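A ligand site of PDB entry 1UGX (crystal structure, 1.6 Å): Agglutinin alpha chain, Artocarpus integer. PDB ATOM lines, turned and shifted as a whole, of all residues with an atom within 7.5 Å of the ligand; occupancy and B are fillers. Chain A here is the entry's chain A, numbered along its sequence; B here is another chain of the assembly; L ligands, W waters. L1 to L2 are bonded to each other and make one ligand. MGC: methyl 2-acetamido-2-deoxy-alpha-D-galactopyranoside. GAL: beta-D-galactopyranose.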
ATOM      1  N   GLY A   1      -6.269  -3.249   3.106  1.00  0.00           N
ATOM      2  CA  GLY A   1      -7.402  -4.119   2.719  1.00  0.00           C
ATOM      3  C   GLY A   1      -7.473  -4.338   1.221  1.00  0.00           C
ATOM      4  O   GLY A   1      -6.641  -3.829   0.466  1.00  0.00           O
ATOM      5  N   LYS A   2      -8.477  -5.096   0.785  1.00  0.00           N
ATOM      6  CA  LYS A   2      -8.658  -5.368  -0.638  1.00  0.00           C
ATOM      7  C   LYS A   2      -9.600  -4.329  -1.225  1.00  0.00           C
ATOM      8  O   LYS A   2     -10.761  -4.253  -0.831  1.00  0.00           O
ATOM      9  CB  LYS A   2      -9.239  -6.769  -0.826  1.00  0.00           C
ATOM     10  CG  LYS A   2      -9.395  -7.173  -2.285  1.00  0.00           C
ATOM     11  CD  LYS A   2      -9.998  -8.571  -2.387  1.00  0.00           C
ATOM     12  CE  LYS A   2     -10.232  -8.970  -3.829  1.00  0.00           C
ATOM     13  NZ  LYS A   2     -10.821 -10.339  -3.923  1.00  0.00           N
ATOM     14  N   ILE A  25     -17.621  -1.947  10.715  1.00  0.00           N
ATOM     15  CA  ILE A  25     -18.342  -2.543   9.594  1.00  0.00           C
ATOM     16  C   ILE A  25     -17.473  -3.607   8.948  1.00  0.00           C
ATOM     17  O   ILE A  25     -16.264  -3.431   8.798  1.00  0.00           O
ATOM     18  CB  ILE A  25     -18.691  -1.476   8.520  1.00  0.00           C
ATOM     19  CG1 ILE A  25     -19.597  -0.400   9.133  1.00  0.00           C
ATOM     20  CG2 ILE A  25     -19.353  -2.147   7.315  1.00  0.00           C
ATOM     21  CD1 ILE A  25     -20.876  -0.935   9.728  1.00  0.00           C
ATOM     22  N   SER A  46     -15.054  -9.311   4.551  1.00  0.00           N
ATOM     23  CA  SER A  46     -13.972  -9.071   5.503  1.00  0.00           C
ATOM     24  C   SER A  46     -13.048 -10.289   5.491  1.00  0.00           C
ATOM     25  O   SER A  46     -13.460 -11.382   5.091  1.00  0.00           O
ATOM     26  CB  SER A  46     -14.569  -8.893   6.911  1.00  0.00           C
ATOM     27  OG  SER A  46     -13.560  -8.968   7.900  1.00  0.00           O
ATOM     28  N   PHE A  47     -11.799 -10.087   5.895  1.00  0.00           N
ATOM     29  CA  PHE A  47     -10.833 -11.186   5.945  1.00  0.00           C
ATOM     30  C   PHE A  47     -11.164 -12.080   7.144  1.00  0.00           C
ATOM     31  O   PHE A  47     -10.699 -13.219   7.210  1.00  0.00           O
ATOM     32  CB  PHE A  47      -9.406 -10.668   6.136  1.00  0.00           C
ATOM     33  CG  PHE A  47      -8.897  -9.804   5.011  1.00  0.00           C
ATOM     34  CD1 PHE A  47      -9.463  -9.870   3.742  1.00  0.00           C
ATOM     35  CD2 PHE A  47      -7.807  -8.975   5.213  1.00  0.00           C
ATOM     36  CE1 PHE A  47      -8.944  -9.116   2.697  1.00  0.00           C
ATOM     37  CE2 PHE A  47      -7.277  -8.212   4.165  1.00  0.00           C
ATOM     38  CZ  PHE A  47      -7.851  -8.287   2.909  1.00  0.00           C
ATOM     39  N   ILE A  48     -11.955 -11.557   8.071  1.00  0.00           N
ATOM     40  CA  ILE A  48     -12.319 -12.318   9.267  1.00  0.00           C
ATOM     41  C   ILE A  48     -13.825 -12.526   9.379  1.00  0.00           C
ATOM     42  O   ILE A  48     -14.585 -12.073   8.529  1.00  0.00           O
ATOM     43  CB  ILE A  48     -11.792 -11.628  10.553  1.00  0.00           C
ATOM     44  CG1 ILE A  48     -12.290 -10.184  10.626  1.00  0.00           C
ATOM     45  CG2 ILE A  48     -10.266 -11.670  10.561  1.00  0.00           C
ATOM     46  CD1 ILE A  48     -11.962  -9.482  11.935  1.00  0.00           C
ATOM     47  N   VAL A  75      -9.382   1.243  15.125  1.00  0.00           N
ATOM     48  CA  VAL A  75      -9.704  -0.082  15.638  1.00  0.00           C
ATOM     49  C   VAL A  75      -8.441  -0.913  15.418  1.00  0.00           C
ATOM     50  O   VAL A  75      -8.013  -1.117  14.282  1.00  0.00           O
ATOM     51  CB  VAL A  75     -10.885  -0.735  14.872  1.00  0.00           C
ATOM     52  CG1 VAL A  75     -11.135  -2.144  15.410  1.00  0.00           C
ATOM     53  CG2 VAL A  75     -12.138   0.115  15.038  1.00  0.00           C
ATOM     54  N   SER A  76      -7.833  -1.363  16.515  1.00  0.00           N
ATOM     55  CA  SER A  76      -6.605  -2.140  16.446  1.00  0.00           C
ATOM     56  C   SER A  76      -5.506  -1.416  15.674  1.00  0.00           C
ATOM     57  O   SER A  76      -4.674  -2.048  15.015  1.00  0.00           O
ATOM     58  CB  SER A  76      -6.880  -3.506  15.813  1.00  0.00           C
ATOM     59  OG  SER A  76      -7.747  -4.263  16.627  1.00  0.00           O
ATOM     60  N   GLY A  77      -5.508  -0.092  15.753  1.00  0.00           N
ATOM     61  CA  GLY A  77      -4.486   0.697  15.080  1.00  0.00           C
ATOM     62  C   GLY A  77      -4.799   1.115  13.653  1.00  0.00           C
ATOM     63  O   GLY A  77      -3.989   1.798  13.025  1.00  0.00           O
ATOM     64  N   TYR A  78      -5.967   0.726  13.149  1.00  0.00           N
ATOM     65  CA  TYR A  78      -6.364   1.070  11.781  1.00  0.00           C
ATOM     66  C   TYR A  78      -7.560   2.003  11.761  1.00  0.00           C
ATOM     67  O   TYR A  78      -8.500   1.831  12.538  1.00  0.00           O
ATOM     68  CB  TYR A  78      -6.737  -0.183  10.996  1.00  0.00           C
ATOM     69  CG  TYR A  78      -5.632  -1.183  10.851  1.00  0.00           C
ATOM     70  CD1 TYR A  78      -4.608  -0.978   9.933  1.00  0.00           C
ATOM     71  CD2 TYR A  78      -5.597  -2.325  11.634  1.00  0.00           C
ATOM     72  CE1 TYR A  78      -3.569  -1.895   9.793  1.00  0.00           C
ATOM     73  CE2 TYR A  78      -4.566  -3.251  11.506  1.00  0.00           C
ATOM     74  CZ  TYR A  78      -3.563  -3.035  10.582  1.00  0.00           C
ATOM     75  OH  TYR A  78      -2.552  -3.959  10.458  1.00  0.00           O
ATOM     76  N   VAL A  79      -7.526   2.989  10.872  1.00  0.00           N
ATOM     77  CA  VAL A  79      -8.654   3.896  10.745  1.00  0.00           C
ATOM     78  C   VAL A  79      -9.645   3.160   9.836  1.00  0.00           C
ATOM     79  O   VAL A  79      -9.284   2.751   8.736  1.00  0.00           O
ATOM     80  CB  VAL A  79      -8.239   5.234  10.089  1.00  0.00           C
ATOM     81  CG1 VAL A  79      -9.453   6.135   9.899  1.00  0.00           C
ATOM     82  CG2 VAL A  79      -7.196   5.926  10.967  1.00  0.00           C
ATOM     83  N   VAL A  80     -10.864   2.971  10.325  1.00  0.00           N
ATOM     84  CA  VAL A  80     -11.893   2.259   9.567  1.00  0.00           C
ATOM     85  C   VAL A  80     -13.257   2.915   9.748  1.00  0.00           C
ATOM     86  O   VAL A  80     -13.425   3.810  10.560  1.00  0.00           O
ATOM     87  CB  VAL A  80     -12.003   0.780  10.014  1.00  0.00           C
ATOM     88  CG1 VAL A  80     -10.694   0.056   9.784  1.00  0.00           C
ATOM     89  CG2 VAL A  80     -12.395   0.716  11.491  1.00  0.00           C
ATOM     90  N   SER A 119     -12.609  -0.198   0.193  1.00  0.00           N
ATOM     91  CA  SER A 119     -11.634  -1.213   0.547  1.00  0.00           C
ATOM     92  C   SER A 119     -12.029  -1.870   1.852  1.00  0.00           C
ATOM     93  O   SER A 119     -12.484  -1.207   2.777  1.00  0.00           O
ATOM     94  CB  SER A 119     -10.261  -0.582   0.689  1.00  0.00           C
ATOM     95  OG  SER A 119      -9.310  -1.523   1.191  1.00  0.00           O
ATOM     96  N   ILE A 120     -11.862  -3.192   1.921  1.00  0.00           N
ATOM     97  CA  ILE A 120     -12.181  -3.925   3.128  1.00  0.00           C
ATOM     98  C   ILE A 120     -11.040  -4.870   3.467  1.00  0.00           C
ATOM     99  O   ILE A 120     -10.555  -5.604   2.607  1.00  0.00           O
ATOM    100  CB  ILE A 120     -13.479  -4.762   2.961  1.00  0.00           C
ATOM    101  CG1 ILE A 120     -14.650  -3.845   2.588  1.00  0.00           C
ATOM    102  CG2 ILE A 120     -13.803  -5.524   4.250  1.00  0.00           C
ATOM    103  CD1 ILE A 120     -15.957  -4.572   2.350  1.00  0.00           C
ATOM    104  N   GLY A 121     -10.602  -4.827   4.722  1.00  0.00           N
ATOM    105  CA  GLY A 121      -9.552  -5.714   5.193  1.00  0.00           C
ATOM    106  C   GLY A 121     -10.271  -6.506   6.272  1.00  0.00           C
ATOM    107  O   GLY A 121     -11.117  -7.332   5.966  1.00  0.00           O
ATOM    108  N   TYR A 122      -9.922  -6.247   7.526  1.00  0.00           N
ATOM    109  CA  TYR A 122     -10.639  -6.908   8.624  1.00  0.00           C
ATOM    110  C   TYR A 122     -11.961  -6.147   8.683  1.00  0.00           C
ATOM    111  O   TYR A 122     -13.018  -6.720   8.943  1.00  0.00           O
ATOM    112  CB  TYR A 122      -9.882  -6.743   9.943  1.00  0.00           C
ATOM    113  CG  TYR A 122      -8.822  -7.784  10.218  1.00  0.00           C
ATOM    114  CD1 TYR A 122      -8.337  -8.601   9.194  1.00  0.00           C
ATOM    115  CD2 TYR A 122      -8.290  -7.947  11.495  1.00  0.00           C
ATOM    116  CE1 TYR A 122      -7.339  -9.549   9.441  1.00  0.00           C
ATOM    117  CE2 TYR A 122      -7.300  -8.894  11.753  1.00  0.00           C
ATOM    118  CZ  TYR A 122      -6.837  -9.689  10.714  1.00  0.00           C
ATOM    119  OH  TYR A 122      -5.840 -10.607  10.951  1.00  0.00           O
ATOM    120  N   TRP A 123     -11.890  -4.853   8.398  1.00  0.00           N
ATOM    121  CA  TRP A 123     -13.069  -3.990   8.426  1.00  0.00           C
ATOM    122  C   TRP A 123     -13.095  -3.096   7.191  1.00  0.00           C
ATOM    123  O   TRP A 123     -12.145  -3.085   6.413  1.00  0.00           O
ATOM    124  CB  TRP A 123     -13.029  -3.111   9.683  1.00  0.00           C
ATOM    125  CG  TRP A 123     -12.916  -3.930  10.920  1.00  0.00           C
ATOM    126  CD1 TRP A 123     -13.879  -4.746  11.447  1.00  0.00           C
ATOM    127  CD2 TRP A 123     -11.741  -4.129  11.720  1.00  0.00           C
ATOM    128  NE1 TRP A 123     -13.382  -5.440  12.528  1.00  0.00           N
ATOM    129  CE2 TRP A 123     -12.068  -5.085  12.714  1.00  0.00           C
ATOM    130  CE3 TRP A 123     -10.442  -3.596  11.693  1.00  0.00           C
ATOM    131  CZ2 TRP A 123     -11.141  -5.527  13.671  1.00  0.00           C
ATOM    132  CZ3 TRP A 123      -9.514  -4.038  12.650  1.00  0.00           C
ATOM    133  CH2 TRP A 123      -9.878  -4.993  13.621  1.00  0.00           C
ATOM    134  N   LEU A 124     -14.190  -2.351   7.027  1.00  0.00           N
ATOM    135  CA  LEU A 124     -14.332  -1.428   5.910  1.00  0.00           C
ATOM    136  C   LEU A 124     -13.344  -0.291   6.164  1.00  0.00           C
ATOM    137  O   LEU A 124     -13.522   0.495   7.100  1.00  0.00           O
ATOM    138  CB  LEU A 124     -15.763  -0.912   5.870  1.00  0.00           C
ATOM    139  CG  LEU A 124     -16.100   0.103   4.774  1.00  0.00           C
ATOM    140  CD1 LEU A 124     -15.850  -0.494   3.402  1.00  0.00           C
ATOM    141  CD2 LEU A 124     -17.550   0.533   4.912  1.00  0.00           C
ATOM    142  N   ASP A 125     -12.297  -0.217   5.343  1.00  0.00           N
ATOM    143  CA  ASP A 125     -11.247   0.794   5.492  1.00  0.00           C
ATOM    144  C   ASP A 125     -11.733   2.180   5.113  1.00  0.00           C
ATOM    145  O   ASP A 125     -11.526   3.151   5.833  1.00  0.00           O
ATOM    146  CB  ASP A 125     -10.046   0.428   4.609  1.00  0.00           C
ATOM    147  CG  ASP A 125      -9.482  -0.944   4.921  1.00  0.00           C
ATOM    148  OD1 ASP A 125      -9.171  -1.205   6.102  1.00  0.00           O
ATOM    149  OD2 ASP A 125      -9.357  -1.757   3.985  1.00  0.00           O
ATOM    150  N   TYR A 126     -12.369   2.251   3.951  1.00  0.00           N
ATOM    151  CA  TYR A 126     -12.891   3.507   3.447  1.00  0.00           C
ATOM    152  C   TYR A 126     -13.871   3.207   2.319  1.00  0.00           C
ATOM    153  O   TYR A 126     -13.921   2.090   1.801  1.00  0.00           O
ATOM    154  CB  TYR A 126     -11.746   4.392   2.931  1.00  0.00           C
ATOM    155  CG  TYR A 126     -10.868   3.751   1.873  1.00  0.00           C
ATOM    156  CD1 TYR A 126     -11.285   3.655   0.541  1.00  0.00           C
ATOM    157  CD2 TYR A 126      -9.609   3.240   2.205  1.00  0.00           C
ATOM    158  CE1 TYR A 126     -10.475   3.051  -0.420  1.00  0.00           C
ATOM    159  CE2 TYR A 126      -8.796   2.645   1.254  1.00  0.00           C
ATOM    160  CZ  TYR A 126      -9.231   2.551  -0.064  1.00  0.00           C
ATOM    161  OH  TYR A 126      -8.416   1.956  -1.006  1.00  0.00           O
ATOM    162  N   GLY B  16     -12.913   7.561   5.754  1.00  0.00           N
ATOM    163  CA  GLY B  16     -12.248   6.450   6.411  1.00  0.00           C
ATOM    164  C   GLY B  16     -10.744   6.618   6.300  1.00  0.00           C
ATOM    165  O   GLY B  16     -10.253   7.752   6.385  1.00  0.00           O
ATOM    166  N   ALA B  17     -10.010   5.529   6.123  1.00  0.00           N
ATOM    167  CA  ALA B  17      -8.563   5.601   6.015  1.00  0.00           C
ATOM    168  C   ALA B  17      -8.133   6.347   4.753  1.00  0.00           C
ATOM    169  O   ALA B  17      -8.818   6.292   3.735  1.00  0.00           O
ATOM    170  CB  ALA B  17      -7.966   4.212   6.012  1.00  0.00           C
ATOM    171  N   LYS B  18      -7.009   7.052   4.815  1.00  0.00           N
ATOM    172  CA  LYS B  18      -6.528   7.786   3.645  1.00  0.00           C
ATOM    173  C   LYS B  18      -5.401   7.026   2.964  1.00  0.00           C
ATOM    174  O   LYS B  18      -5.596   6.529   1.830  1.00  0.00           O
ATOM    175  CB  LYS B  18      -6.062   9.177   4.063  1.00  0.00           C
ATOM    176  CG  LYS B  18      -7.190  10.170   4.294  1.00  0.00           C
ATOM    177  CD  LYS B  18      -6.672  11.583   4.332  1.00  0.00           C
ATOM    178  CE  LYS B  18      -7.806  12.575   4.483  1.00  0.00           C
ATOM    179  NZ  LYS B  18      -7.304  13.966   4.360  1.00  0.00           N
HETATM  180  O6  MGC L   1      -9.479  -3.353   7.873  1.00  0.00           O
HETATM  181  C6  MGC L   1      -8.403  -2.964   8.703  1.00  0.00           C
HETATM  182  C5  MGC L   1      -7.048  -3.543   8.268  1.00  0.00           C
HETATM  183  O5  MGC L   1      -7.144  -5.034   7.975  1.00  0.00           O
HETATM  184  C1  MGC L   1      -5.894  -5.737   7.564  1.00  0.00           C
HETATM  185  O1  MGC L   1      -4.988  -5.754   8.677  1.00  0.00           O
HETATM  186  CM  MGC L   1      -5.397  -6.450  10.026  1.00  0.00           C
HETATM  187  C2  MGC L   1      -5.301  -5.020   6.349  1.00  0.00           C
HETATM  188  N2  MGC L   1      -4.149  -5.785   6.071  1.00  0.00           N
HETATM  189  C7  MGC L   1      -3.757  -6.169   4.821  1.00  0.00           C
HETATM  190  O7  MGC L   1      -4.525  -6.218   3.841  1.00  0.00           O
HETATM  191  C8  MGC L   1      -2.295  -6.550   4.628  1.00  0.00           C
HETATM  192  C3  MGC L   1      -5.087  -3.535   6.667  1.00  0.00           C
HETATM  193  O3  MGC L   1      -4.523  -2.935   5.541  1.00  0.00           O
HETATM  194  C4  MGC L   1      -6.465  -2.837   6.963  1.00  0.00           C
HETATM  195  O4  MGC L   1      -7.304  -3.065   5.805  1.00  0.00           O
HETATM  196  C1  GAL L   2      -3.491  -1.937   5.469  1.00  0.00           C
HETATM  197  C2  GAL L   2      -2.686  -1.845   4.189  1.00  0.00           C
HETATM  198  C3  GAL L   2      -1.845  -0.572   4.198  1.00  0.00           C
HETATM  199  C4  GAL L   2      -2.788   0.728   4.287  1.00  0.00           C
HETATM  200  C5  GAL L   2      -3.615   0.638   5.612  1.00  0.00           C
HETATM  201  C6  GAL L   2      -4.639   1.590   6.189  1.00  0.00           C
HETATM  202  O2  GAL L   2      -1.896  -3.025   4.113  1.00  0.00           O
HETATM  203  O3  GAL L   2      -1.089  -0.507   2.981  1.00  0.00           O
HETATM  204  O4  GAL L   2      -3.728   0.768   3.201  1.00  0.00           O
HETATM  205  O5  GAL L   2      -4.345  -0.711   5.620  1.00  0.00           O
HETATM  206  O6  GAL L   2      -5.450   1.637   7.357  1.00  0.00           O
HETATM  207  O   HOH W   1      -1.810  -5.465   7.979  1.00  0.00           O
HETATM  208  O   HOH W   2      -3.378  -3.934   1.838  1.00  0.00           O
HETATM  209  O   HOH W   3      -7.825   0.721   7.545  1.00  0.00           O
HETATM  210  O   HOH W   4      -0.399  -3.575   6.789  1.00  0.00           O
HETATM  211  O   HOH W   5      -4.681  -6.684   0.981  1.00  0.00           O
HETATM  212  O   HOH W   6      -5.193   3.631   9.005  1.00  0.00           O
HETATM  213  O   HOH W   7      -6.245  -0.679   2.224  1.00  0.00           O
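N of Phe 47 is in hydrogen-bond range of O of Gly 121, at 2.8 Å. The backbone carbonyl oxygen (O) of Tyr 122 sits at hydrogen-bond distance from the side-chain hydroxyl (OG) of Ser 46, at 2.5 Å. The side-chain carboxylate (OD2) of Asp 125 sits at hydrogen-bond distance from the backbone NH (N) of Gly 121 (3.4 Å). The backbone carbonyl oxygen (O) of Asp 125 sits at hydrogen-bond distance from the backbone NH (N) of Ala 17 of chain B. The backbone NH of Asp 125 lies within hydrogen-bond range of the backbone carbonyl oxygen of Ser 119, at 2.8 Å.
Water W3 lies within hydrogen-bond range of O6 of GAL L2 (2.6 Å), OD1 of Asp 125 (2.8 Å) and O of Val 79 (2.8 Å). Water W6 bridges an oxygen (O6) of GAL L2 and the backbone NH of Val 79. Water W2 bridges an oxygen (O2) of GAL L2 (2.9 Å) and the backbone NH (N) of Gly 1 (3.2 Å). Water W1 bridges OH of Tyr 78 (3.0 Å) and N2 of MGC L1 (3.0 Å). Water W7 lies within hydrogen-bond range of N of Gly 1, O4 of GAL L2 and OG of Ser 119.
The side-chain carboxylate (OD1) of Asp 125 lies within hydrogen-bond range of an oxygen (O4) of MGC L1, 2.7 Å away. An oxygen (O4) of MGC L1 lies within hydrogen-bond range of the backbone NH (N) of Gly 1 (2.9 Å). O6 of MGC L1 sits at hydrogen-bond distance from N of Tyr 122 (2.9 Å). The backbone NH of Trp 123 lies within hydrogen-bond range of an oxygen (O6) of MGC L1, 2.9 Å away. The backbone carbonyl oxygen (O) of Trp 123 is in hydrogen-bond range of an oxygen (O6) of MGC L1 (3.1 Å).
Merely in contact with the ligand: Phe 47 (3.4 Å), Tyr 78 (3.5 Å), Gly 121 (3.5 Å), Ala 17 of chain B (3.8 Å) and Val 80 (3.9 Å). Nine residues have an atom within 4 Å of the ligand: Gly 1, Phe 47, Tyr 78, Val 80, Gly 121, Tyr 122, Trp 123, Asp 125 and Ala 17 of chain B. The nearest printed residue that does not touch the ligand is Val 79 (4.2 Å).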
